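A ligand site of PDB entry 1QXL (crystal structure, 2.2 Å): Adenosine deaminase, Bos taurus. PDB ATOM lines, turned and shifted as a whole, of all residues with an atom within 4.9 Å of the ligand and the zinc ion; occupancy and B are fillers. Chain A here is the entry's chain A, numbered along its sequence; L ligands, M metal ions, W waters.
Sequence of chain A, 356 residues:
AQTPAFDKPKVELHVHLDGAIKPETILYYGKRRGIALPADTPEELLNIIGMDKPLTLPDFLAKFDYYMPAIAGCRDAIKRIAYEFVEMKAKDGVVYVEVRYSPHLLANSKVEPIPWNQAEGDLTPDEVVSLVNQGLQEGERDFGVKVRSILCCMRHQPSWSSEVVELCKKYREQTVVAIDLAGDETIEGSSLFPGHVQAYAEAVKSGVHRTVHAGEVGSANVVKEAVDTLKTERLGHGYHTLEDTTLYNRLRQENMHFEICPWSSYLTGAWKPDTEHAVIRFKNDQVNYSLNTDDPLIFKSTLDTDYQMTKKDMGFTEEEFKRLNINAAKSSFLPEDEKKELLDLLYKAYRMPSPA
Of the 26 residues printed, 4 come within 4 Å of the zinc ion. Along chain A the residues within 4 Å of the zinc ion span positions 14 to 294.
Water W3 lies within hydrogen-bond range of the side-chain carboxylate of Asp 294 (2.6 Å), a ring nitrogen (NE2) of His 237 (2.8 Å) and a nitrogen (N3) of the ligand (3.4 Å). Water W6 lies within hydrogen-bond range of the side-chain carboxylate of Glu 216 (2.5 Å) and an oxygen (O1) of the ligand (2.7 Å). Water W1 lies within hydrogen-bond range of N of Gly 183 and O1 of the ligand. Water W5 lies within hydrogen-bond range of the side-chain carboxylate (OE2) of Glu 216 (2.7 Å), a nitrogen (N3) of the ligand (2.9 Å) and the side-chain carboxylate (OD2) of Asp 294 (3.0 Å). Water W2 bridges the side-chain carboxylate of Asp 184 (3.2 Å) and an oxygen (O3) of the ligand (3.5 Å).
The zinc ion is bound by NE2 of His 16 (1.9 Å), water W3 (2.0 Å), NE2 of His 14 (2.0 Å), NE2 of His 213 (2.3 Å) and OD1 of Asp 294 (2.5 Å). The zinc ion has five donor atoms within binding distance.
O of Leu 55 touches C24 of the ligand, 3.5 Å away. Thr 56 touches the ligand. N of Leu 57 touches C24 of the ligand, 3.7 Å away. Phe 60 touches the ligand. Leu 61 touches the ligand (CD2 to C12, 3.7 Å). CZ of Phe 64 touches C2 of the ligand, 3.7 Å away. CD1 of Leu 105 touches C7 of the ligand (3.9 Å). Met 154 touches the ligand (CE to C10, 3.8 Å). CA of Gly 183 touches C15 of the ligand (3.4 Å). Glu 216 touches the ligand. Val 217 touches the ligand. Thr 268 touches the ligand (CB to C27, 3.7 Å). Hydrophobic or aromatic side chains within 4 Å of the ligand: His 16, Leu 57, Phe 60, Leu 61, Phe 64, Leu 105, Met 154 and Val 217. The nearest printed residue that does not touch the ligand is Tyr 101 (4.05 Å).
ND1 of His 16 lies within hydrogen-bond range of O2 of the ligand (2.6 Å). A nitrogen (N2) of the ligand lies within hydrogen-bond range of the side-chain carboxylate of Asp 295. OD2 of Asp 18 sits at hydrogen-bond distance from O2 of the ligand, 2.7 Å away. The backbone NH (N) of Asp 184 sits at hydrogen-bond distance from an oxygen (O3) of the ligand (3.0 Å).
NH1 of Arg 100 is in hydrogen-bond range of ND1 of His 14. A ring nitrogen (NE2) of His 237 lies close to the side-chain carboxylate of Glu 216 (3.4 Å). N of Leu 105 lies within hydrogen-bond range of OG of Ser 102, at 3.2 Å. O of Leu 105 sits at hydrogen-bond distance from NE1 of Trp 116 (2.7 Å).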
ATOM      1  N   HIS A  14       7.947  16.907  35.104  1.00  0.00           N
ATOM      2  CA  HIS A  14       7.031  16.720  33.953  1.00  0.00           C
ATOM      3  C   HIS A  14       7.142  15.359  33.276  1.00  0.00           C
ATOM      4  O   HIS A  14       7.937  15.120  32.371  1.00  0.00           O
ATOM      5  CB  HIS A  14       7.201  17.811  32.849  1.00  0.00           C
ATOM      6  CG  HIS A  14       6.084  17.794  31.821  1.00  0.00           C
ATOM      7  ND1 HIS A  14       5.353  18.852  31.514  1.00  0.00           N
ATOM      8  CD2 HIS A  14       5.673  16.818  30.937  1.00  0.00           C
ATOM      9  CE1 HIS A  14       4.508  18.595  30.497  1.00  0.00           C
ATOM     10  NE2 HIS A  14       4.695  17.296  30.099  1.00  0.00           N
ATOM     11  N   HIS A  16       4.315  11.963  32.404  1.00  0.00           N
ATOM     12  CA  HIS A  16       2.990  11.312  32.472  1.00  0.00           C
ATOM     13  C   HIS A  16       3.000   9.827  32.913  1.00  0.00           C
ATOM     14  O   HIS A  16       3.566   8.968  32.251  1.00  0.00           O
ATOM     15  CB  HIS A  16       2.346  11.380  31.052  1.00  0.00           C
ATOM     16  CG  HIS A  16       2.090  12.825  30.538  1.00  0.00           C
ATOM     17  ND1 HIS A  16       0.919  13.474  30.588  1.00  0.00           N
ATOM     18  CD2 HIS A  16       2.983  13.699  29.922  1.00  0.00           C
ATOM     19  CE1 HIS A  16       1.036  14.702  30.023  1.00  0.00           C
ATOM     20  NE2 HIS A  16       2.327  14.879  29.607  1.00  0.00           N
ATOM     21  N   ASP A  18       0.811   7.528  32.593  1.00  0.00           N
ATOM     22  CA  ASP A  18       0.206   6.706  31.565  1.00  0.00           C
ATOM     23  C   ASP A  18       0.980   6.585  30.282  1.00  0.00           C
ATOM     24  O   ASP A  18       0.559   5.899  29.379  1.00  0.00           O
ATOM     25  CB  ASP A  18      -1.289   7.133  31.253  1.00  0.00           C
ATOM     26  CG  ASP A  18      -1.450   8.603  30.881  1.00  0.00           C
ATOM     27  OD1 ASP A  18      -2.523   8.953  30.395  1.00  0.00           O
ATOM     28  OD2 ASP A  18      -0.534   9.384  31.082  1.00  0.00           O
ATOM     29  N   LEU A  55       5.644  10.981  13.925  1.00  0.00           N
ATOM     30  CA  LEU A  55       4.422  10.605  13.202  1.00  0.00           C
ATOM     31  C   LEU A  55       3.361  11.677  13.300  1.00  0.00           C
ATOM     32  O   LEU A  55       3.517  12.672  13.946  1.00  0.00           O
ATOM     33  CB  LEU A  55       3.721   9.401  13.831  1.00  0.00           C
ATOM     34  CG  LEU A  55       4.560   8.452  14.668  1.00  0.00           C
ATOM     35  CD1 LEU A  55       3.625   7.791  15.666  1.00  0.00           C
ATOM     36  CD2 LEU A  55       5.363   7.423  13.862  1.00  0.00           C
ATOM     37  N   THR A  56       2.204  11.414  12.732  1.00  0.00           N
ATOM     38  CA  THR A  56       1.097  12.349  12.984  1.00  0.00           C
ATOM     39  C   THR A  56       0.308  12.196  14.247  1.00  0.00           C
ATOM     40  O   THR A  56       0.369  11.203  14.937  1.00  0.00           O
ATOM     41  CB  THR A  56       0.023  12.167  11.952  1.00  0.00           C
ATOM     42  OG1 THR A  56      -0.634  10.864  12.081  1.00  0.00           O
ATOM     43  CG2 THR A  56       0.693  12.350  10.615  1.00  0.00           C
ATOM     44  N   LEU A  57      -0.524  13.199  14.513  1.00  0.00           N
ATOM     45  CA  LEU A  57      -1.303  13.104  15.750  1.00  0.00           C
ATOM     46  C   LEU A  57      -2.152  11.818  15.962  1.00  0.00           C
ATOM     47  O   LEU A  57      -2.127  11.176  16.996  1.00  0.00           O
ATOM     48  CB  LEU A  57      -2.091  14.413  15.925  1.00  0.00           C
ATOM     49  CG  LEU A  57      -2.163  15.103  17.303  1.00  0.00           C
ATOM     50  CD1 LEU A  57      -3.454  15.846  17.478  1.00  0.00           C
ATOM     51  CD2 LEU A  57      -2.006  14.181  18.513  1.00  0.00           C
ATOM     52  N   PHE A  60      -0.023   9.118  16.763  1.00  0.00           N
ATOM     53  CA  PHE A  60       0.385   9.194  18.187  1.00  0.00           C
ATOM     54  C   PHE A  60      -0.651   8.706  19.175  1.00  0.00           C
ATOM     55  O   PHE A  60      -0.371   7.966  20.112  1.00  0.00           O
ATOM     56  CB  PHE A  60       0.961  10.587  18.476  1.00  0.00           C
ATOM     57  CG  PHE A  60       1.431  10.880  19.896  1.00  0.00           C
ATOM     58  CD1 PHE A  60       2.746  10.551  20.287  1.00  0.00           C
ATOM     59  CD2 PHE A  60       0.571  11.559  20.798  1.00  0.00           C
ATOM     60  CE1 PHE A  60       3.172  10.838  21.590  1.00  0.00           C
ATOM     61  CE2 PHE A  60       1.002  11.838  22.104  1.00  0.00           C
ATOM     62  CZ  PHE A  60       2.294  11.438  22.508  1.00  0.00           C
ATOM     63  N   LEU A  61      -1.913   9.092  18.892  1.00  0.00           N
ATOM     64  CA  LEU A  61      -2.961   8.641  19.813  1.00  0.00           C
ATOM     65  C   LEU A  61      -3.335   7.120  19.877  1.00  0.00           C
ATOM     66  O   LEU A  61      -3.738   6.516  20.869  1.00  0.00           O
ATOM     67  CB  LEU A  61      -4.164   9.530  19.543  1.00  0.00           C
ATOM     68  CG  LEU A  61      -3.976  11.057  19.807  1.00  0.00           C
ATOM     69  CD1 LEU A  61      -5.364  11.702  19.873  1.00  0.00           C
ATOM     70  CD2 LEU A  61      -3.251  11.484  21.108  1.00  0.00           C
ATOM     71  N   PHE A  64      -1.781   5.022  22.455  1.00  0.00           N
ATOM     72  CA  PHE A  64      -2.624   4.919  23.652  1.00  0.00           C
ATOM     73  C   PHE A  64      -3.703   3.828  23.585  1.00  0.00           C
ATOM     74  O   PHE A  64      -3.973   3.049  24.509  1.00  0.00           O
ATOM     75  CB  PHE A  64      -3.164   6.328  24.007  1.00  0.00           C
ATOM     76  CG  PHE A  64      -2.060   7.263  24.475  1.00  0.00           C
ATOM     77  CD1 PHE A  64      -1.631   8.338  23.667  1.00  0.00           C
ATOM     78  CD2 PHE A  64      -1.462   7.051  25.755  1.00  0.00           C
ATOM     79  CE1 PHE A  64      -0.541   9.163  24.111  1.00  0.00           C
ATOM     80  CE2 PHE A  64      -0.408   7.857  26.207  1.00  0.00           C
ATOM     81  CZ  PHE A  64       0.065   8.864  25.358  1.00  0.00           C
ATOM     82  N   ARG A 100       2.090  13.221  36.626  1.00  0.00           N
ATOM     83  CA  ARG A 100       0.789  13.694  36.144  1.00  0.00           C
ATOM     84  C   ARG A 100       0.025  12.680  35.307  1.00  0.00           C
ATOM     85  O   ARG A 100       0.581  11.794  34.629  1.00  0.00           O
ATOM     86  CB  ARG A 100       1.071  14.950  35.355  1.00  0.00           C
ATOM     87  CG  ARG A 100       1.562  14.733  33.923  1.00  0.00           C
ATOM     88  CD  ARG A 100       1.829  16.068  33.269  1.00  0.00           C
ATOM     89  NE  ARG A 100       2.706  16.806  34.152  1.00  0.00           N
ATOM     90  CZ  ARG A 100       3.002  18.093  34.047  1.00  0.00           C
ATOM     91  NH1 ARG A 100       2.370  18.860  33.189  1.00  0.00           N
ATOM     92  NH2 ARG A 100       3.976  18.624  34.758  1.00  0.00           N
ATOM     93  N   TYR A 101      -1.285  12.783  35.389  1.00  0.00           N
ATOM     94  CA  TYR A 101      -2.183  11.869  34.679  1.00  0.00           C
ATOM     95  C   TYR A 101      -3.598  12.376  34.789  1.00  0.00           C
ATOM     96  O   TYR A 101      -4.037  13.019  35.744  1.00  0.00           O
ATOM     97  CB  TYR A 101      -2.086  10.381  35.268  1.00  0.00           C
ATOM     98  CG  TYR A 101      -2.659  10.254  36.703  1.00  0.00           C
ATOM     99  CD1 TYR A 101      -3.979   9.793  36.845  1.00  0.00           C
ATOM    100  CD2 TYR A 101      -1.895  10.638  37.830  1.00  0.00           C
ATOM    101  CE1 TYR A 101      -4.569   9.727  38.103  1.00  0.00           C
ATOM    102  CE2 TYR A 101      -2.495  10.586  39.105  1.00  0.00           C
ATOM    103  CZ  TYR A 101      -3.800  10.084  39.221  1.00  0.00           C
ATOM    104  OH  TYR A 101      -4.375   9.953  40.455  1.00  0.00           O
ATOM    105  N   SER A 102      -4.362  12.024  33.786  1.00  0.00           N
ATOM    106  CA  SER A 102      -5.853  12.144  33.852  1.00  0.00           C
ATOM    107  C   SER A 102      -6.591  10.963  34.500  1.00  0.00           C
ATOM    108  O   SER A 102      -6.613   9.858  34.010  1.00  0.00           O
ATOM    109  CB  SER A 102      -6.478  12.241  32.470  1.00  0.00           C
ATOM    110  OG  SER A 102      -7.913  12.100  32.527  1.00  0.00           O
ATOM    111  N   LEU A 105      -9.260   9.242  32.313  1.00  0.00           N
ATOM    112  CA  LEU A 105      -8.795   8.277  31.286  1.00  0.00           C
ATOM    113  C   LEU A 105      -8.448   6.847  31.708  1.00  0.00           C
ATOM    114  O   LEU A 105      -8.242   5.953  30.891  1.00  0.00           O
ATOM    115  CB  LEU A 105      -7.594   8.746  30.497  1.00  0.00           C
ATOM    116  CG  LEU A 105      -7.801  10.098  29.765  1.00  0.00           C
ATOM    117  CD1 LEU A 105      -6.575  10.414  28.969  1.00  0.00           C
ATOM    118  CD2 LEU A 105      -9.052  10.134  28.845  1.00  0.00           C
ATOM    119  N   TRP A 116     -11.361   4.770  25.824  1.00  0.00           N
ATOM    120  CA  TRP A 116     -10.771   3.550  25.175  1.00  0.00           C
ATOM    121  C   TRP A 116     -11.719   2.490  24.578  1.00  0.00           C
ATOM    122  O   TRP A 116     -11.396   1.317  24.514  1.00  0.00           O
ATOM    123  CB  TRP A 116      -9.786   2.804  26.115  1.00  0.00           C
ATOM    124  CG  TRP A 116      -8.973   3.851  26.788  1.00  0.00           C
ATOM    125  CD1 TRP A 116      -8.876   4.104  28.142  1.00  0.00           C
ATOM    126  CD2 TRP A 116      -8.112   4.815  26.136  1.00  0.00           C
ATOM    127  NE1 TRP A 116      -8.011   5.114  28.358  1.00  0.00           N
ATOM    128  CE2 TRP A 116      -7.494   5.584  27.169  1.00  0.00           C
ATOM    129  CE3 TRP A 116      -7.828   5.095  24.772  1.00  0.00           C
ATOM    130  CZ2 TRP A 116      -6.562   6.568  26.847  1.00  0.00           C
ATOM    131  CZ3 TRP A 116      -6.907   6.112  24.456  1.00  0.00           C
ATOM    132  CH2 TRP A 116      -6.247   6.831  25.486  1.00  0.00           C
ATOM    133  N   CYS A 152      -4.528  15.746  35.518  1.00  0.00           N
ATOM    134  CA  CYS A 152      -4.591  16.499  34.282  1.00  0.00           C
ATOM    135  C   CYS A 152      -6.026  16.773  33.941  1.00  0.00           C
ATOM    136  O   CYS A 152      -6.780  15.822  33.782  1.00  0.00           O
ATOM    137  CB  CYS A 152      -4.072  15.674  33.096  1.00  0.00           C
ATOM    138  SG  CYS A 152      -2.284  15.479  33.257  1.00  0.00           S
ATOM    139  N   MET A 154      -8.271  17.570  30.577  1.00  0.00           N
ATOM    140  CA  MET A 154      -8.120  17.411  29.082  1.00  0.00           C
ATOM    141  C   MET A 154      -8.707  18.514  28.116  1.00  0.00           C
ATOM    142  O   MET A 154      -9.879  18.816  28.162  1.00  0.00           O
ATOM    143  CB  MET A 154      -8.621  16.019  28.607  1.00  0.00           C
ATOM    144  CG  MET A 154      -7.990  14.873  29.362  1.00  0.00           C
ATOM    145  SD  MET A 154      -6.259  14.888  28.953  1.00  0.00           S
ATOM    146  CE  MET A 154      -6.405  14.464  27.237  1.00  0.00           C
ATOM    147  N   HIS A 156      -9.989  18.934  25.112  1.00  0.00           N
ATOM    148  CA  HIS A 156     -11.202  18.510  24.440  1.00  0.00           C
ATOM    149  C   HIS A 156     -12.389  18.233  25.323  1.00  0.00           C
ATOM    150  O   HIS A 156     -13.490  17.940  24.891  1.00  0.00           O
ATOM    151  CB  HIS A 156     -10.883  17.342  23.452  1.00  0.00           C
ATOM    152  CG  HIS A 156     -10.717  15.969  24.110  1.00  0.00           C
ATOM    153  ND1 HIS A 156      -9.605  15.517  24.709  1.00  0.00           N
ATOM    154  CD2 HIS A 156     -11.693  14.965  24.228  1.00  0.00           C
ATOM    155  CE1 HIS A 156      -9.881  14.264  25.219  1.00  0.00           C
ATOM    156  NE2 HIS A 156     -11.172  13.924  24.921  1.00  0.00           N
ATOM    157  N   GLY A 183      -3.426  17.743  26.457  1.00  0.00           N
ATOM    158  CA  GLY A 183      -4.041  17.137  25.276  1.00  0.00           C
ATOM    159  C   GLY A 183      -4.225  18.019  24.073  1.00  0.00           C
ATOM    160  O   GLY A 183      -5.352  18.147  23.677  1.00  0.00           O
ATOM    161  N   ASP A 184      -3.289  18.619  23.411  1.00  0.00           N
ATOM    162  CA  ASP A 184      -3.875  19.152  22.063  1.00  0.00           C
ATOM    163  C   ASP A 184      -4.331  20.589  22.057  1.00  0.00           C
ATOM    164  O   ASP A 184      -5.473  20.970  21.844  1.00  0.00           O
ATOM    165  CB  ASP A 184      -4.891  18.390  21.073  1.00  0.00           C
ATOM    166  CG  ASP A 184      -4.934  18.980  19.620  1.00  0.00           C
ATOM    167  OD1 ASP A 184      -3.997  19.658  19.293  1.00  0.00           O
ATOM    168  OD2 ASP A 184      -5.852  18.792  18.829  1.00  0.00           O
ATOM    169  N   HIS A 213       0.007  22.660  29.819  1.00  0.00           N
ATOM    170  CA  HIS A 213       0.861  22.448  28.669  1.00  0.00           C
ATOM    171  C   HIS A 213       0.600  23.491  27.589  1.00  0.00           C
ATOM    172  O   HIS A 213      -0.535  23.665  27.167  1.00  0.00           O
ATOM    173  CB  HIS A 213       0.541  21.131  27.996  1.00  0.00           C
ATOM    174  CG  HIS A 213       0.891  19.836  28.706  1.00  0.00           C
ATOM    175  ND1 HIS A 213       0.323  19.380  29.779  1.00  0.00           N
ATOM    176  CD2 HIS A 213       1.790  18.877  28.278  1.00  0.00           C
ATOM    177  CE1 HIS A 213       0.828  18.178  30.060  1.00  0.00           C
ATOM    178  NE2 HIS A 213       1.746  17.839  29.128  1.00  0.00           N
ATOM    179  N   GLU A 216       3.962  23.791  23.123  1.00  0.00           N
ATOM    180  CA  GLU A 216       4.687  22.657  22.556  1.00  0.00           C
ATOM    181  C   GLU A 216       4.582  22.608  21.019  1.00  0.00           C
ATOM    182  O   GLU A 216       5.552  22.568  20.274  1.00  0.00           O
ATOM    183  CB  GLU A 216       4.234  21.306  23.156  1.00  0.00           C
ATOM    184  CG  GLU A 216       4.885  19.981  22.664  1.00  0.00           C
ATOM    185  CD  GLU A 216       4.160  18.780  23.249  1.00  0.00           C
ATOM    186  OE1 GLU A 216       3.110  18.955  23.871  1.00  0.00           O
ATOM    187  OE2 GLU A 216       4.647  17.660  23.126  1.00  0.00           O
ATOM    188  N   VAL A 217       3.314  22.666  20.640  1.00  0.00           N
ATOM    189  CA  VAL A 217       2.940  22.695  19.203  1.00  0.00           C
ATOM    190  C   VAL A 217       1.926  23.871  18.879  1.00  0.00           C
ATOM    191  O   VAL A 217       1.402  24.082  17.798  1.00  0.00           O
ATOM    192  CB  VAL A 217       2.430  21.223  18.982  1.00  0.00           C
ATOM    193  CG1 VAL A 217       0.961  21.018  19.086  1.00  0.00           C
ATOM    194  CG2 VAL A 217       3.195  20.303  18.023  1.00  0.00           C
ATOM    195  N   HIS A 237       6.450  22.651  28.530  1.00  0.00           N
ATOM    196  CA  HIS A 237       7.244  22.987  27.381  1.00  0.00           C
ATOM    197  C   HIS A 237       7.505  24.520  27.194  1.00  0.00           C
ATOM    198  O   HIS A 237       8.551  25.098  27.464  1.00  0.00           O
ATOM    199  CB  HIS A 237       6.585  22.442  26.089  1.00  0.00           C
ATOM    200  CG  HIS A 237       6.325  20.951  26.143  1.00  0.00           C
ATOM    201  ND1 HIS A 237       7.241  20.007  25.833  1.00  0.00           N
ATOM    202  CD2 HIS A 237       5.138  20.282  26.453  1.00  0.00           C
ATOM    203  CE1 HIS A 237       6.703  18.775  25.926  1.00  0.00           C
ATOM    204  NE2 HIS A 237       5.407  18.953  26.317  1.00  0.00           N
ATOM    205  N   THR A 268       8.530  14.143  18.828  1.00  0.00           N
ATOM    206  CA  THR A 268       7.186  14.616  18.403  1.00  0.00           C
ATOM    207  C   THR A 268       7.033  15.525  17.189  1.00  0.00           C
ATOM    208  O   THR A 268       5.933  15.743  16.730  1.00  0.00           O
ATOM    209  CB  THR A 268       6.416  15.368  19.478  1.00  0.00           C
ATOM    210  OG1 THR A 268       6.981  16.689  19.707  1.00  0.00           O
ATOM    211  CG2 THR A 268       6.275  14.528  20.780  1.00  0.00           C
ATOM    212  N   ASP A 294       8.867  13.307  30.126  1.00  0.00           N
ATOM    213  CA  ASP A 294       7.511  13.304  29.517  1.00  0.00           C
ATOM    214  C   ASP A 294       6.783  11.973  29.381  1.00  0.00           C
ATOM    215  O   ASP A 294       5.815  11.704  30.087  1.00  0.00           O
ATOM    216  CB  ASP A 294       7.532  14.117  28.212  1.00  0.00           C
ATOM    217  CG  ASP A 294       6.240  14.734  27.723  1.00  0.00           C
ATOM    218  OD1 ASP A 294       5.299  14.795  28.472  1.00  0.00           O
ATOM    219  OD2 ASP A 294       6.172  15.211  26.585  1.00  0.00           O
ATOM    220  N   ASP A 295       7.286  11.163  28.441  1.00  0.00           N
ATOM    221  CA  ASP A 295       6.683   9.835  28.249  1.00  0.00           C
ATOM    222  C   ASP A 295       7.730   8.770  27.911  1.00  0.00           C
ATOM    223  O   ASP A 295       7.894   8.407  26.754  1.00  0.00           O
ATOM    224  CB  ASP A 295       5.717   9.776  27.032  1.00  0.00           C
ATOM    225  CG  ASP A 295       4.586  10.825  27.065  1.00  0.00           C
ATOM    226  OD1 ASP A 295       3.519  10.479  27.603  1.00  0.00           O
ATOM    227  OD2 ASP A 295       4.827  11.927  26.524  1.00  0.00           O
HETATM  228  C1  LIG L   1      -0.664  13.074  27.080  1.00  0.00           C
HETATM  229  N1  LIG L   1      -0.909  11.942  27.976  1.00  0.00           N
HETATM  230  C2  LIG L   1       0.235  11.278  28.123  1.00  0.00           C
HETATM  231  N2  LIG L   1       1.234  11.887  27.476  1.00  0.00           N
HETATM  232  C3  LIG L   1       0.625  13.006  26.744  1.00  0.00           C
HETATM  233  C4  LIG L   1       1.330  13.893  25.781  1.00  0.00           C
HETATM  234  O1  LIG L   1       0.723  14.735  25.134  1.00  0.00           O
HETATM  235  N3  LIG L   1       2.629  13.783  25.671  1.00  0.00           N
HETATM  236  C5  LIG L   1      -2.197  11.554  28.509  1.00  0.00           C
HETATM  237  C6  LIG L   1      -2.441  12.121  29.942  1.00  0.00           C
HETATM  238  O2  LIG L   1      -1.199  11.977  30.752  1.00  0.00           O
HETATM  239  C7  LIG L   1      -3.313  11.948  27.515  1.00  0.00           C
HETATM  240  C8  LIG L   1      -3.379  11.025  26.266  1.00  0.00           C
HETATM  241  N4  LIG L   1      -4.398  11.617  25.344  1.00  0.00           N
HETATM  242  C9  LIG L   1      -5.694  11.220  25.178  1.00  0.00           C
HETATM  243  C10 LIG L   1      -6.317  12.047  24.245  1.00  0.00           C
HETATM  244  C11 LIG L   1      -5.337  13.008  23.806  1.00  0.00           C
HETATM  245  C12 LIG L   1      -4.135  12.686  24.507  1.00  0.00           C
HETATM  246  C13 LIG L   1      -5.368  14.047  22.926  1.00  0.00           C
HETATM  247  C14 LIG L   1      -4.229  14.807  22.715  1.00  0.00           C
HETATM  248  C15 LIG L   1      -3.031  14.493  23.412  1.00  0.00           C
HETATM  249  C16 LIG L   1      -3.011  13.421  24.292  1.00  0.00           C
HETATM  250  N5  LIG L   1      -1.876  15.195  23.330  1.00  0.00           N
HETATM  251  C17 LIG L   1      -1.591  16.072  22.377  1.00  0.00           C
HETATM  252  O3  LIG L   1      -2.344  16.531  21.545  1.00  0.00           O
HETATM  253  C18 LIG L   1      -0.142  16.473  22.421  1.00  0.00           C
HETATM  254  C19 LIG L   1       0.565  16.175  21.094  1.00  0.00           C
HETATM  255  C20 LIG L   1       2.117  16.552  18.041  1.00  0.00           C
HETATM  256  C21 LIG L   1       2.608  15.640  18.973  1.00  0.00           C
HETATM  257  C22 LIG L   1       2.830  14.329  18.611  1.00  0.00           C
HETATM  258  C23 LIG L   1       2.676  13.966  17.290  1.00  0.00           C
HETATM  259  C24 LIG L   1       2.242  14.896  16.345  1.00  0.00           C
HETATM  260  C25 LIG L   1       1.934  16.193  16.713  1.00  0.00           C
HETATM  261  C26 LIG L   1       1.931  15.586  21.346  1.00  0.00           C
HETATM  262  C27 LIG L   1       2.939  16.084  20.334  1.00  0.00           C
HETATM  263 ZN    ZN M   1       3.423  16.322  28.892  1.00  0.00          ZN
HETATM  264  O   HOH W   1      -1.082  16.386  26.527  1.00  0.00           O
HETATM  265  O   HOH W   2      -1.195  18.228  18.736  1.00  0.00           O
HETATM  266  O   HOH W   3       3.986  16.585  26.994  1.00  0.00           O
HETATM  267  O   HOH W   4       3.464  15.879  13.322  1.00  0.00           O
HETATM  268  O   HOH W   5       4.650  15.076  23.955  1.00  0.00           O
HETATM  269  O   HOH W   6       1.656  17.239  24.934  1.00  0.00           O
